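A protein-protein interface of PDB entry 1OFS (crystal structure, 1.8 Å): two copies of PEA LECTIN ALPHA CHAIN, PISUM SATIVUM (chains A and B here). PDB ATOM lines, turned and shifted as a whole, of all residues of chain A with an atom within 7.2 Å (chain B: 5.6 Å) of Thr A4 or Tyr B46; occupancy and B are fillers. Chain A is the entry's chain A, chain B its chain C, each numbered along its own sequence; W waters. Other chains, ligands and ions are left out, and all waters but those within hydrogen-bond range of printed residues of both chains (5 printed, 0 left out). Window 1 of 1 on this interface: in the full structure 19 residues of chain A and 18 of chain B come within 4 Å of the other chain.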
ATOM      1  N   GLU A   2      11.480  10.776  -8.876  1.00  0.00           N
ATOM      2  CA  GLU A   2      10.258  10.450  -8.165  1.00  0.00           C
ATOM      3  C   GLU A   2       9.767  11.655  -7.394  1.00  0.00           C
ATOM      4  O   GLU A   2      10.565  12.393  -6.824  1.00  0.00           O
ATOM      5  CB  GLU A   2      10.521   9.320  -7.168  1.00  0.00           C
ATOM      6  CG  GLU A   2      10.420   7.926  -7.752  1.00  0.00           C
ATOM      7  CD  GLU A   2      11.171   6.902  -6.925  1.00  0.00           C
ATOM      8  OE1 GLU A   2      12.362   6.665  -7.220  1.00  0.00           O
ATOM      9  OE2 GLU A   2      10.574   6.336  -5.986  1.00  0.00           O
ATOM     10  N   THR A   3       8.457  11.872  -7.407  1.00  0.00           N
ATOM     11  CA  THR A   3       7.872  12.950  -6.627  1.00  0.00           C
ATOM     12  C   THR A   3       6.592  12.430  -5.997  1.00  0.00           C
ATOM     13  O   THR A   3       5.935  11.533  -6.539  1.00  0.00           O
ATOM     14  CB  THR A   3       7.582  14.225  -7.458  1.00  0.00           C
ATOM     15  OG1 THR A   3       6.476  13.998  -8.347  1.00  0.00           O
ATOM     16  CG2 THR A   3       8.743  14.565  -8.386  1.00  0.00           C
ATOM     17  N   THR A   4       6.276  12.963  -4.824  1.00  0.00           N
ATOM     18  CA  THR A   4       5.051  12.618  -4.131  1.00  0.00           C
ATOM     19  C   THR A   4       4.503  13.921  -3.609  1.00  0.00           C
ATOM     20  O   THR A   4       5.244  14.727  -3.061  1.00  0.00           O
ATOM     21  CB  THR A   4       5.336  11.706  -2.934  1.00  0.00           C
ATOM     22  OG1 THR A   4       5.766  10.422  -3.394  1.00  0.00           O
ATOM     23  CG2 THR A   4       4.043  11.415  -2.178  1.00  0.00           C
ATOM     24  N   SER A   5       3.211  14.156  -3.777  1.00  0.00           N
ATOM     25  CA  SER A   5       2.641  15.381  -3.236  1.00  0.00           C
ATOM     26  C   SER A   5       1.183  15.177  -2.915  1.00  0.00           C
ATOM     27  O   SER A   5       0.533  14.276  -3.460  1.00  0.00           O
ATOM     28  CB  SER A   5       2.782  16.569  -4.200  1.00  0.00           C
ATOM     29  OG  SER A   5       3.758  16.341  -5.203  1.00  0.00           O
ATOM     30  N   PHE A   6       0.673  16.014  -2.020  1.00  0.00           N
ATOM     31  CA  PHE A   6      -0.739  15.973  -1.672  1.00  0.00           C
ATOM     32  C   PHE A   6      -1.108  17.268  -0.984  1.00  0.00           C
ATOM     33  O   PHE A   6      -0.242  17.978  -0.475  1.00  0.00           O
ATOM     34  CB  PHE A   6      -1.092  14.760  -0.803  1.00  0.00           C
ATOM     35  CG  PHE A   6      -0.501  14.796   0.576  1.00  0.00           C
ATOM     36  CD1 PHE A   6      -1.151  15.459   1.610  1.00  0.00           C
ATOM     37  CD2 PHE A   6       0.685  14.139   0.851  1.00  0.00           C
ATOM     38  CE1 PHE A   6      -0.619  15.476   2.888  1.00  0.00           C
ATOM     39  CE2 PHE A   6       1.227  14.152   2.128  1.00  0.00           C
ATOM     40  CZ  PHE A   6       0.572  14.817   3.149  1.00  0.00           C
ATOM     41  N   TYR A  46       0.448   9.950   6.481  1.00  0.00           N
ATOM     42  CA  TYR A  46       0.033   9.936   5.085  1.00  0.00           C
ATOM     43  C   TYR A  46       0.083   8.465   4.664  1.00  0.00           C
ATOM     44  O   TYR A  46       1.052   7.761   4.945  1.00  0.00           O
ATOM     45  CB  TYR A  46       0.944  10.804   4.216  1.00  0.00           C
ATOM     46  CG  TYR A  46       0.459  10.882   2.786  1.00  0.00           C
ATOM     47  CD1 TYR A  46      -0.837  11.308   2.495  1.00  0.00           C
ATOM     48  CD2 TYR A  46       1.277  10.502   1.732  1.00  0.00           C
ATOM     49  CE1 TYR A  46      -1.294  11.367   1.188  1.00  0.00           C
ATOM     50  CE2 TYR A  46       0.828  10.556   0.420  1.00  0.00           C
ATOM     51  CZ  TYR A  46      -0.452  10.999   0.155  1.00  0.00           C
ATOM     52  OH  TYR A  46      -0.896  11.057  -1.149  1.00  0.00           O
ATOM     53  N   SER A  47      -0.958   8.001   3.982  1.00  0.00           N
ATOM     54  CA  SER A  47      -1.041   6.591   3.591  1.00  0.00           C
ATOM     55  C   SER A  47       0.108   6.049   2.734  1.00  0.00           C
ATOM     56  O   SER A  47       0.579   4.930   2.953  1.00  0.00           O
ATOM     57  CB  SER A  47      -2.392   6.327   2.912  1.00  0.00           C
ATOM     58  OG  SER A  47      -2.487   7.066   1.717  1.00  0.00           O
ATOM     59  N   SER A  48       0.573   6.833   1.775  1.00  0.00           N
ATOM     60  CA  SER A  48       1.647   6.356   0.910  1.00  0.00           C
ATOM     61  C   SER A  48       3.059   6.538   1.447  1.00  0.00           C
ATOM     62  O   SER A  48       3.435   7.625   1.895  1.00  0.00           O
ATOM     63  CB  SER A  48       1.595   7.039  -0.460  1.00  0.00           C
ATOM     64  OG  SER A  48       2.607   6.519  -1.317  1.00  0.00           O
ATOM     65  N   PRO A  49       3.834   5.462   1.420  1.00  0.00           N
ATOM     66  CA  PRO A  49       5.242   5.552   1.796  1.00  0.00           C
ATOM     67  C   PRO A  49       5.877   6.604   0.876  1.00  0.00           C
ATOM     68  O   PRO A  49       5.397   6.789  -0.245  1.00  0.00           O
ATOM     69  CB  PRO A  49       5.771   4.156   1.467  1.00  0.00           C
ATOM     70  CG  PRO A  49       4.575   3.256   1.634  1.00  0.00           C
ATOM     71  CD  PRO A  49       3.428   4.081   1.097  1.00  0.00           C
ATOM     72  N   ILE A  50       6.913   7.293   1.349  1.00  0.00           N
ATOM     73  CA  ILE A  50       7.609   8.320   0.577  1.00  0.00           C
ATOM     74  C   ILE A  50       9.064   7.893   0.401  1.00  0.00           C
ATOM     75  O   ILE A  50       9.682   7.404   1.344  1.00  0.00           O
ATOM     76  CB  ILE A  50       7.556   9.679   1.307  1.00  0.00           C
ATOM     77  CG1 ILE A  50       6.116  10.038   1.689  1.00  0.00           C
ATOM     78  CG2 ILE A  50       8.176  10.784   0.445  1.00  0.00           C
ATOM     79  CD1 ILE A  50       5.180  10.098   0.516  1.00  0.00           C
ATOM     80  N   HIS A  51       9.607   8.092  -0.799  1.00  0.00           N
ATOM     81  CA  HIS A  51      10.989   7.716  -1.087  1.00  0.00           C
ATOM     82  C   HIS A  51      11.889   8.890  -0.714  1.00  0.00           C
ATOM     83  O   HIS A  51      11.924   9.899  -1.418  1.00  0.00           O
ATOM     84  CB  HIS A  51      11.126   7.354  -2.573  1.00  0.00           C
ATOM     85  CG  HIS A  51      12.239   6.398  -2.870  1.00  0.00           C
ATOM     86  ND1 HIS A  51      12.398   5.804  -4.106  1.00  0.00           N
ATOM     87  CD2 HIS A  51      13.250   5.938  -2.098  1.00  0.00           C
ATOM     88  CE1 HIS A  51      13.454   5.009  -4.076  1.00  0.00           C
ATOM     89  NE2 HIS A  51      13.989   5.073  -2.872  1.00  0.00           N
ATOM     90  N   PHE A  63      12.342  18.147   0.081  1.00  0.00           N
ATOM     91  CA  PHE A  63      10.916  18.114   0.383  1.00  0.00           C
ATOM     92  C   PHE A  63      10.508  19.322   1.181  1.00  0.00           C
ATOM     93  O   PHE A  63      11.346  20.007   1.772  1.00  0.00           O
ATOM     94  CB  PHE A  63      10.474  16.804   1.078  1.00  0.00           C
ATOM     95  CG  PHE A  63      11.014  16.625   2.474  1.00  0.00           C
ATOM     96  CD1 PHE A  63      10.437  17.289   3.548  1.00  0.00           C
ATOM     97  CD2 PHE A  63      12.092  15.781   2.709  1.00  0.00           C
ATOM     98  CE1 PHE A  63      10.935  17.116   4.844  1.00  0.00           C
ATOM     99  CE2 PHE A  63      12.592  15.604   3.996  1.00  0.00           C
ATOM    100  CZ  PHE A  63      12.014  16.272   5.060  1.00  0.00           C
ATOM    101  N   VAL A  64       9.215  19.609   1.144  1.00  0.00           N
ATOM    102  CA  VAL A  64       8.660  20.722   1.893  1.00  0.00           C
ATOM    103  C   VAL A  64       7.272  20.295   2.346  1.00  0.00           C
ATOM    104  O   VAL A  64       6.569  19.555   1.646  1.00  0.00           O
ATOM    105  CB  VAL A  64       8.578  22.029   1.048  1.00  0.00           C
ATOM    106  CG1 VAL A  64       7.885  21.767  -0.290  1.00  0.00           C
ATOM    107  CG2 VAL A  64       7.895  23.162   1.823  1.00  0.00           C
ATOM    108  N   THR B   4      -4.015  14.737  -4.942  1.00  0.00           N
ATOM    109  CA  THR B   4      -3.098  13.626  -4.788  1.00  0.00           C
ATOM    110  C   THR B   4      -2.247  13.617  -6.043  1.00  0.00           C
ATOM    111  O   THR B   4      -2.783  13.667  -7.142  1.00  0.00           O
ATOM    112  CB  THR B   4      -3.852  12.301  -4.704  1.00  0.00           C
ATOM    113  OG1 THR B   4      -4.551  12.220  -3.461  1.00  0.00           O
ATOM    114  CG2 THR B   4      -2.875  11.130  -4.642  1.00  0.00           C
ATOM    115  N   SER B   5      -0.929  13.569  -5.900  1.00  0.00           N
ATOM    116  CA  SER B   5      -0.083  13.515  -7.092  1.00  0.00           C
ATOM    117  C   SER B   5       1.164  12.688  -6.850  1.00  0.00           C
ATOM    118  O   SER B   5       1.603  12.523  -5.712  1.00  0.00           O
ATOM    119  CB  SER B   5       0.318  14.911  -7.593  1.00  0.00           C
ATOM    120  OG  SER B   5      -0.560  15.928  -7.137  1.00  0.00           O
ATOM    121  N   PHE B   6       1.708  12.141  -7.930  1.00  0.00           N
ATOM    122  CA  PHE B   6       2.954  11.384  -7.853  1.00  0.00           C
ATOM    123  C   PHE B   6       3.538  11.232  -9.243  1.00  0.00           C
ATOM    124  O   PHE B   6       2.826  11.381 -10.243  1.00  0.00           O
ATOM    125  CB  PHE B   6       2.775  10.023  -7.160  1.00  0.00           C
ATOM    126  CG  PHE B   6       1.976   9.016  -7.956  1.00  0.00           C
ATOM    127  CD1 PHE B   6       2.595   8.204  -8.904  1.00  0.00           C
ATOM    128  CD2 PHE B   6       0.616   8.857  -7.731  1.00  0.00           C
ATOM    129  CE1 PHE B   6       1.875   7.271  -9.618  1.00  0.00           C
ATOM    130  CE2 PHE B   6      -0.116   7.925  -8.453  1.00  0.00           C
ATOM    131  CZ  PHE B   6       0.519   7.124  -9.396  1.00  0.00           C
ATOM    132  N   LEU B   7       4.843  10.975  -9.284  1.00  0.00           N
ATOM    133  CA  LEU B   7       5.567  10.766 -10.525  1.00  0.00           C
ATOM    134  C   LEU B   7       6.650   9.728 -10.280  1.00  0.00           C
ATOM    135  O   LEU B   7       7.327   9.750  -9.246  1.00  0.00           O
ATOM    136  CB  LEU B   7       6.210  12.063 -11.028  1.00  0.00           C
ATOM    137  CG  LEU B   7       7.367  11.804 -12.018  1.00  0.00           C
ATOM    138  CD1 LEU B   7       6.817  11.496 -13.414  1.00  0.00           C
ATOM    139  CD2 LEU B   7       8.353  12.941 -12.057  1.00  0.00           C
ATOM    140  N   ASN B  17       5.657   2.508  -2.718  1.00  0.00           N
ATOM    141  CA  ASN B  17       4.427   3.298  -2.862  1.00  0.00           C
ATOM    142  C   ASN B  17       3.435   2.648  -3.830  1.00  0.00           C
ATOM    143  O   ASN B  17       2.433   3.254  -4.193  1.00  0.00           O
ATOM    144  CB  ASN B  17       4.687   4.770  -3.218  1.00  0.00           C
ATOM    145  CG  ASN B  17       5.528   4.943  -4.462  1.00  0.00           C
ATOM    146  OD1 ASN B  17       6.046   3.976  -5.036  1.00  0.00           O
ATOM    147  ND2 ASN B  17       5.669   6.192  -4.895  1.00  0.00           N
ATOM    148  N   LEU B  18       3.736   1.418  -4.246  1.00  0.00           N
ATOM    149  CA  LEU B  18       2.858   0.652  -5.130  1.00  0.00           C
ATOM    150  C   LEU B  18       2.442  -0.660  -4.464  1.00  0.00           C
ATOM    151  O   LEU B  18       3.176  -1.216  -3.639  1.00  0.00           O
ATOM    152  CB  LEU B  18       3.537   0.334  -6.470  1.00  0.00           C
ATOM    153  CG  LEU B  18       3.997   1.507  -7.345  1.00  0.00           C
ATOM    154  CD1 LEU B  18       4.616   0.998  -8.661  1.00  0.00           C
ATOM    155  CD2 LEU B  18       2.860   2.470  -7.610  1.00  0.00           C
ATOM    156  N   ILE B  19       1.253  -1.142  -4.819  1.00  0.00           N
ATOM    157  CA  ILE B  19       0.746  -2.405  -4.317  1.00  0.00           C
ATOM    158  C   ILE B  19       0.750  -3.332  -5.511  1.00  0.00           C
ATOM    159  O   ILE B  19       0.160  -3.013  -6.553  1.00  0.00           O
ATOM    160  CB  ILE B  19      -0.691  -2.270  -3.768  1.00  0.00           C
ATOM    161  CG1 ILE B  19      -0.726  -1.331  -2.561  1.00  0.00           C
ATOM    162  CG2 ILE B  19      -1.222  -3.635  -3.353  1.00  0.00           C
ATOM    163  CD1 ILE B  19      -2.141  -0.916  -2.154  1.00  0.00           C
ATOM    164  N   ALA B  44      -0.819  -3.502 -10.604  1.00  0.00           N
ATOM    165  CA  ALA B  44      -0.031  -2.619  -9.757  1.00  0.00           C
ATOM    166  C   ALA B  44      -0.905  -1.413  -9.487  1.00  0.00           C
ATOM    167  O   ALA B  44      -1.425  -0.794 -10.412  1.00  0.00           O
ATOM    168  CB  ALA B  44       1.264  -2.210 -10.447  1.00  0.00           C
ATOM    169  N   LEU B  45      -1.096  -1.098  -8.212  1.00  0.00           N
ATOM    170  CA  LEU B  45      -1.938   0.024  -7.829  1.00  0.00           C
ATOM    171  C   LEU B  45      -1.169   1.032  -7.002  1.00  0.00           C
ATOM    172  O   LEU B  45      -0.228   0.667  -6.296  1.00  0.00           O
ATOM    173  CB  LEU B  45      -3.117  -0.488  -6.997  1.00  0.00           C
ATOM    174  CG  LEU B  45      -4.046  -1.476  -7.716  1.00  0.00           C
ATOM    175  CD1 LEU B  45      -3.636  -2.916  -7.447  1.00  0.00           C
ATOM    176  CD2 LEU B  45      -5.490  -1.237  -7.311  1.00  0.00           C
ATOM    177  N   TYR B  46      -1.561   2.302  -7.084  1.00  0.00           N
ATOM    178  CA  TYR B  46      -0.905   3.306  -6.254  1.00  0.00           C
ATOM    179  C   TYR B  46      -1.344   3.064  -4.806  1.00  0.00           C
ATOM    180  O   TYR B  46      -2.512   2.745  -4.535  1.00  0.00           O
ATOM    181  CB  TYR B  46      -1.229   4.730  -6.704  1.00  0.00           C
ATOM    182  CG  TYR B  46      -0.437   5.761  -5.943  1.00  0.00           C
ATOM    183  CD1 TYR B  46       0.961   5.750  -5.964  1.00  0.00           C
ATOM    184  CD2 TYR B  46      -1.074   6.737  -5.190  1.00  0.00           C
ATOM    185  CE1 TYR B  46       1.693   6.689  -5.258  1.00  0.00           C
ATOM    186  CE2 TYR B  46      -0.345   7.683  -4.483  1.00  0.00           C
ATOM    187  CZ  TYR B  46       1.033   7.657  -4.528  1.00  0.00           C
ATOM    188  OH  TYR B  46       1.755   8.598  -3.824  1.00  0.00           O
ATOM    189  N   SER B  47      -0.400   3.196  -3.878  1.00  0.00           N
ATOM    190  CA  SER B  47      -0.671   2.932  -2.471  1.00  0.00           C
ATOM    191  C   SER B  47      -1.790   3.767  -1.832  1.00  0.00           C
ATOM    192  O   SER B  47      -2.615   3.231  -1.099  1.00  0.00           O
ATOM    193  CB  SER B  47       0.625   3.061  -1.653  1.00  0.00           C
ATOM    194  OG  SER B  47       0.371   3.002  -0.262  1.00  0.00           O
ATOM    195  N   SER B  48      -1.823   5.064  -2.104  1.00  0.00           N
ATOM    196  CA  SER B  48      -2.838   5.903  -1.479  1.00  0.00           C
ATOM    197  C   SER B  48      -4.201   5.870  -2.130  1.00  0.00           C
ATOM    198  O   SER B  48      -4.317   5.927  -3.350  1.00  0.00           O
ATOM    199  CB  SER B  48      -2.399   7.370  -1.450  1.00  0.00           C
ATOM    200  OG  SER B  48      -3.476   8.180  -0.988  1.00  0.00           O
ATOM    201  N   PRO B  49      -5.238   5.716  -1.318  1.00  0.00           N
ATOM    202  CA  PRO B  49      -6.596   5.829  -1.839  1.00  0.00           C
ATOM    203  C   PRO B  49      -6.705   7.249  -2.397  1.00  0.00           C
ATOM    204  O   PRO B  49      -6.017   8.176  -1.926  1.00  0.00           O
ATOM    205  CB  PRO B  49      -7.459   5.623  -0.593  1.00  0.00           C
ATOM    206  CG  PRO B  49      -6.610   4.701   0.247  1.00  0.00           C
ATOM    207  CD  PRO B  49      -5.221   5.312   0.101  1.00  0.00           C
ATOM    208  N   ILE B  50      -7.546   7.411  -3.408  1.00  0.00           N
ATOM    209  CA  ILE B  50      -7.727   8.688  -4.072  1.00  0.00           C
ATOM    210  C   ILE B  50      -9.175   9.137  -3.955  1.00  0.00           C
ATOM    211  O   ILE B  50     -10.093   8.351  -4.185  1.00  0.00           O
ATOM    212  CB  ILE B  50      -7.299   8.551  -5.542  1.00  0.00           C
ATOM    213  CG1 ILE B  50      -5.778   8.377  -5.622  1.00  0.00           C
ATOM    214  CG2 ILE B  50      -7.726   9.762  -6.349  1.00  0.00           C
ATOM    215  CD1 ILE B  50      -5.294   7.841  -6.946  1.00  0.00           C
HETATM  216  O   HOH W   1       8.284   7.389  -5.076  1.00  0.00           O
HETATM  217  O   HOH W   2      -3.486  11.005  -1.414  1.00  0.00           O
HETATM  218  O   HOH W   3       6.610   8.703  -6.616  1.00  0.00           O
HETATM  219  O   HOH W   4       4.396   8.122  -2.961  1.00  0.00           O
HETATM  220  O   HOH W   5       0.696  10.925  -3.282  1.00  0.00           O
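The side-chain hydroxyl of Ser A47 lies within hydrogen-bond range of the side-chain hydroxyl of Ser B48, 3.1 Å away.
The side-chain hydroxyl (OH) of Tyr B46 lies within hydrogen-bond range of the side-chain hydroxyl (OG) of Ser A48 (3.4 Å).
The backbone carbonyl oxygen (O) of Thr A3 sits at hydrogen-bond distance from the backbone NH (N) of Leu B7 (3.0 Å).
The backbone carbonyl oxygen (O) of Ser A5 sits at hydrogen-bond distance from the backbone NH (N) of Ser B5 (2.9 Å).
The backbone NH (N) of Ser B47 lies within hydrogen-bond range of the backbone carbonyl oxygen (O) of Asn B17 (2.9 Å).
The side-chain carboxylate (OE2) of Glu A2 lies within hydrogen-bond range of a ring nitrogen (ND1) of His A51 (2.7 Å).
Among the printed residues, merely in contact across the chains: Glu A2 with Leu B7 (3.2 Å), Thr A3 with Phe B6 (3.3 Å), Ser A48 with Asn B17 (3.3 Å), Pro A49 with Ser B47 (3.5 Å), Ser A47 with Pro B49 (3.6 Å), Pro A49 with Asn B17 (3.7 Å), Ser A47 with Ser B47 (3.8 Å), Ser A48 with Ser B47 (3.8 Å), Thr A4 with Ser B5 (3.8 Å), Ser A5 with Thr B4 (3.9 Å), Tyr A46 with Ser B48 (3.9 Å) and Thr A4 with Tyr B46 (3.98 Å).
Of the printed residues of chain B, Thr A3 touches Phe B6 and Leu B7.
Of the printed residues of chain B, Thr A4 touches Ser B5 (3.8 Å) and Tyr B46 (3.98 Å).
Printed residues of chain B within 4 Å of Pro A49: Asn B17 (3.7 Å) and Ser B47 (3.5 Å).
Of the printed residues of chain A, Leu B7 touches Glu A2 (3.2 Å) and Thr A3 (3.0 Å).
Of the printed residues of chain A, Tyr B46 touches Thr A4 and Ser A48.
Printed residues of chain A within 4 Å of Pro B49: Ser A47 (3.6 Å).
The nearest printed residue of chain A that does not touch Tyr B46 is Tyr A46 (4.5 Å).
The nearest printed residue of chain A that does not touch Ser B47 is Tyr A46 (7.1 Å).
Hydrophobic or aromatic side chains of chain A within 4 Å of the printed part of chain B: Tyr A46 and Pro A49.
Of the 14 printed residues of chain B, 9 touch a printed residue of chain A.
Printed residues of chain B that touch a printed residue of chain A: Thr B4, Ser B5, Phe B6, Leu B7, Asn B17, Tyr B46, Ser B47, Ser B48 and Pro B49.
Among the printed residues, 16 pairs touch across the chains.
Thr A4 touches Ser B5, and with the chains exchanged Ser A5 touches Thr B4.
Thr A4 touches Tyr B46, but with the chains exchanged Tyr A46 does not touch Thr B4 (4.02 Å).
Ser A5 touches its own counterpart, Ser B5.
Tyr A46 touches Ser B48, and with the chains exchanged Ser A48 touches Tyr B46.
Water W2 lies within hydrogen-bond range of the side-chain hydroxyl of Tyr A46 (2.6 Å), the side-chain hydroxyl of Thr B4 (2.6 Å) and the side-chain hydroxyl of Ser B48 (2.9 Å).
Water W5 lies within hydrogen-bond range of OH of Tyr B46 (2.6 Å), OH of Tyr A46 (2.7 Å), O of Ser B5 (3.0 Å) and O of Ser A5 (3.4 Å).
Water W1 lies within hydrogen-bond range of the side-chain carboxylate of Glu A2 (2.7 Å) and the side-chain amide nitrogen of Asn B17 (2.9 Å).
Water W4 lies within hydrogen-bond range of OG1 of Thr A4 (2.7 Å), OH of Tyr B46 (2.8 Å), OG of Ser A48 (2.9 Å), ND2 of Asn B17 (3.0 Å) and O of Pro A49 (3.2 Å).
Water W3 lies within hydrogen-bond range of the backbone carbonyl oxygen of Thr A3 (2.9 Å), the backbone carbonyl oxygen of Leu B7 (2.9 Å) and the side-chain amide nitrogen of Asn B17 (3.2 Å).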
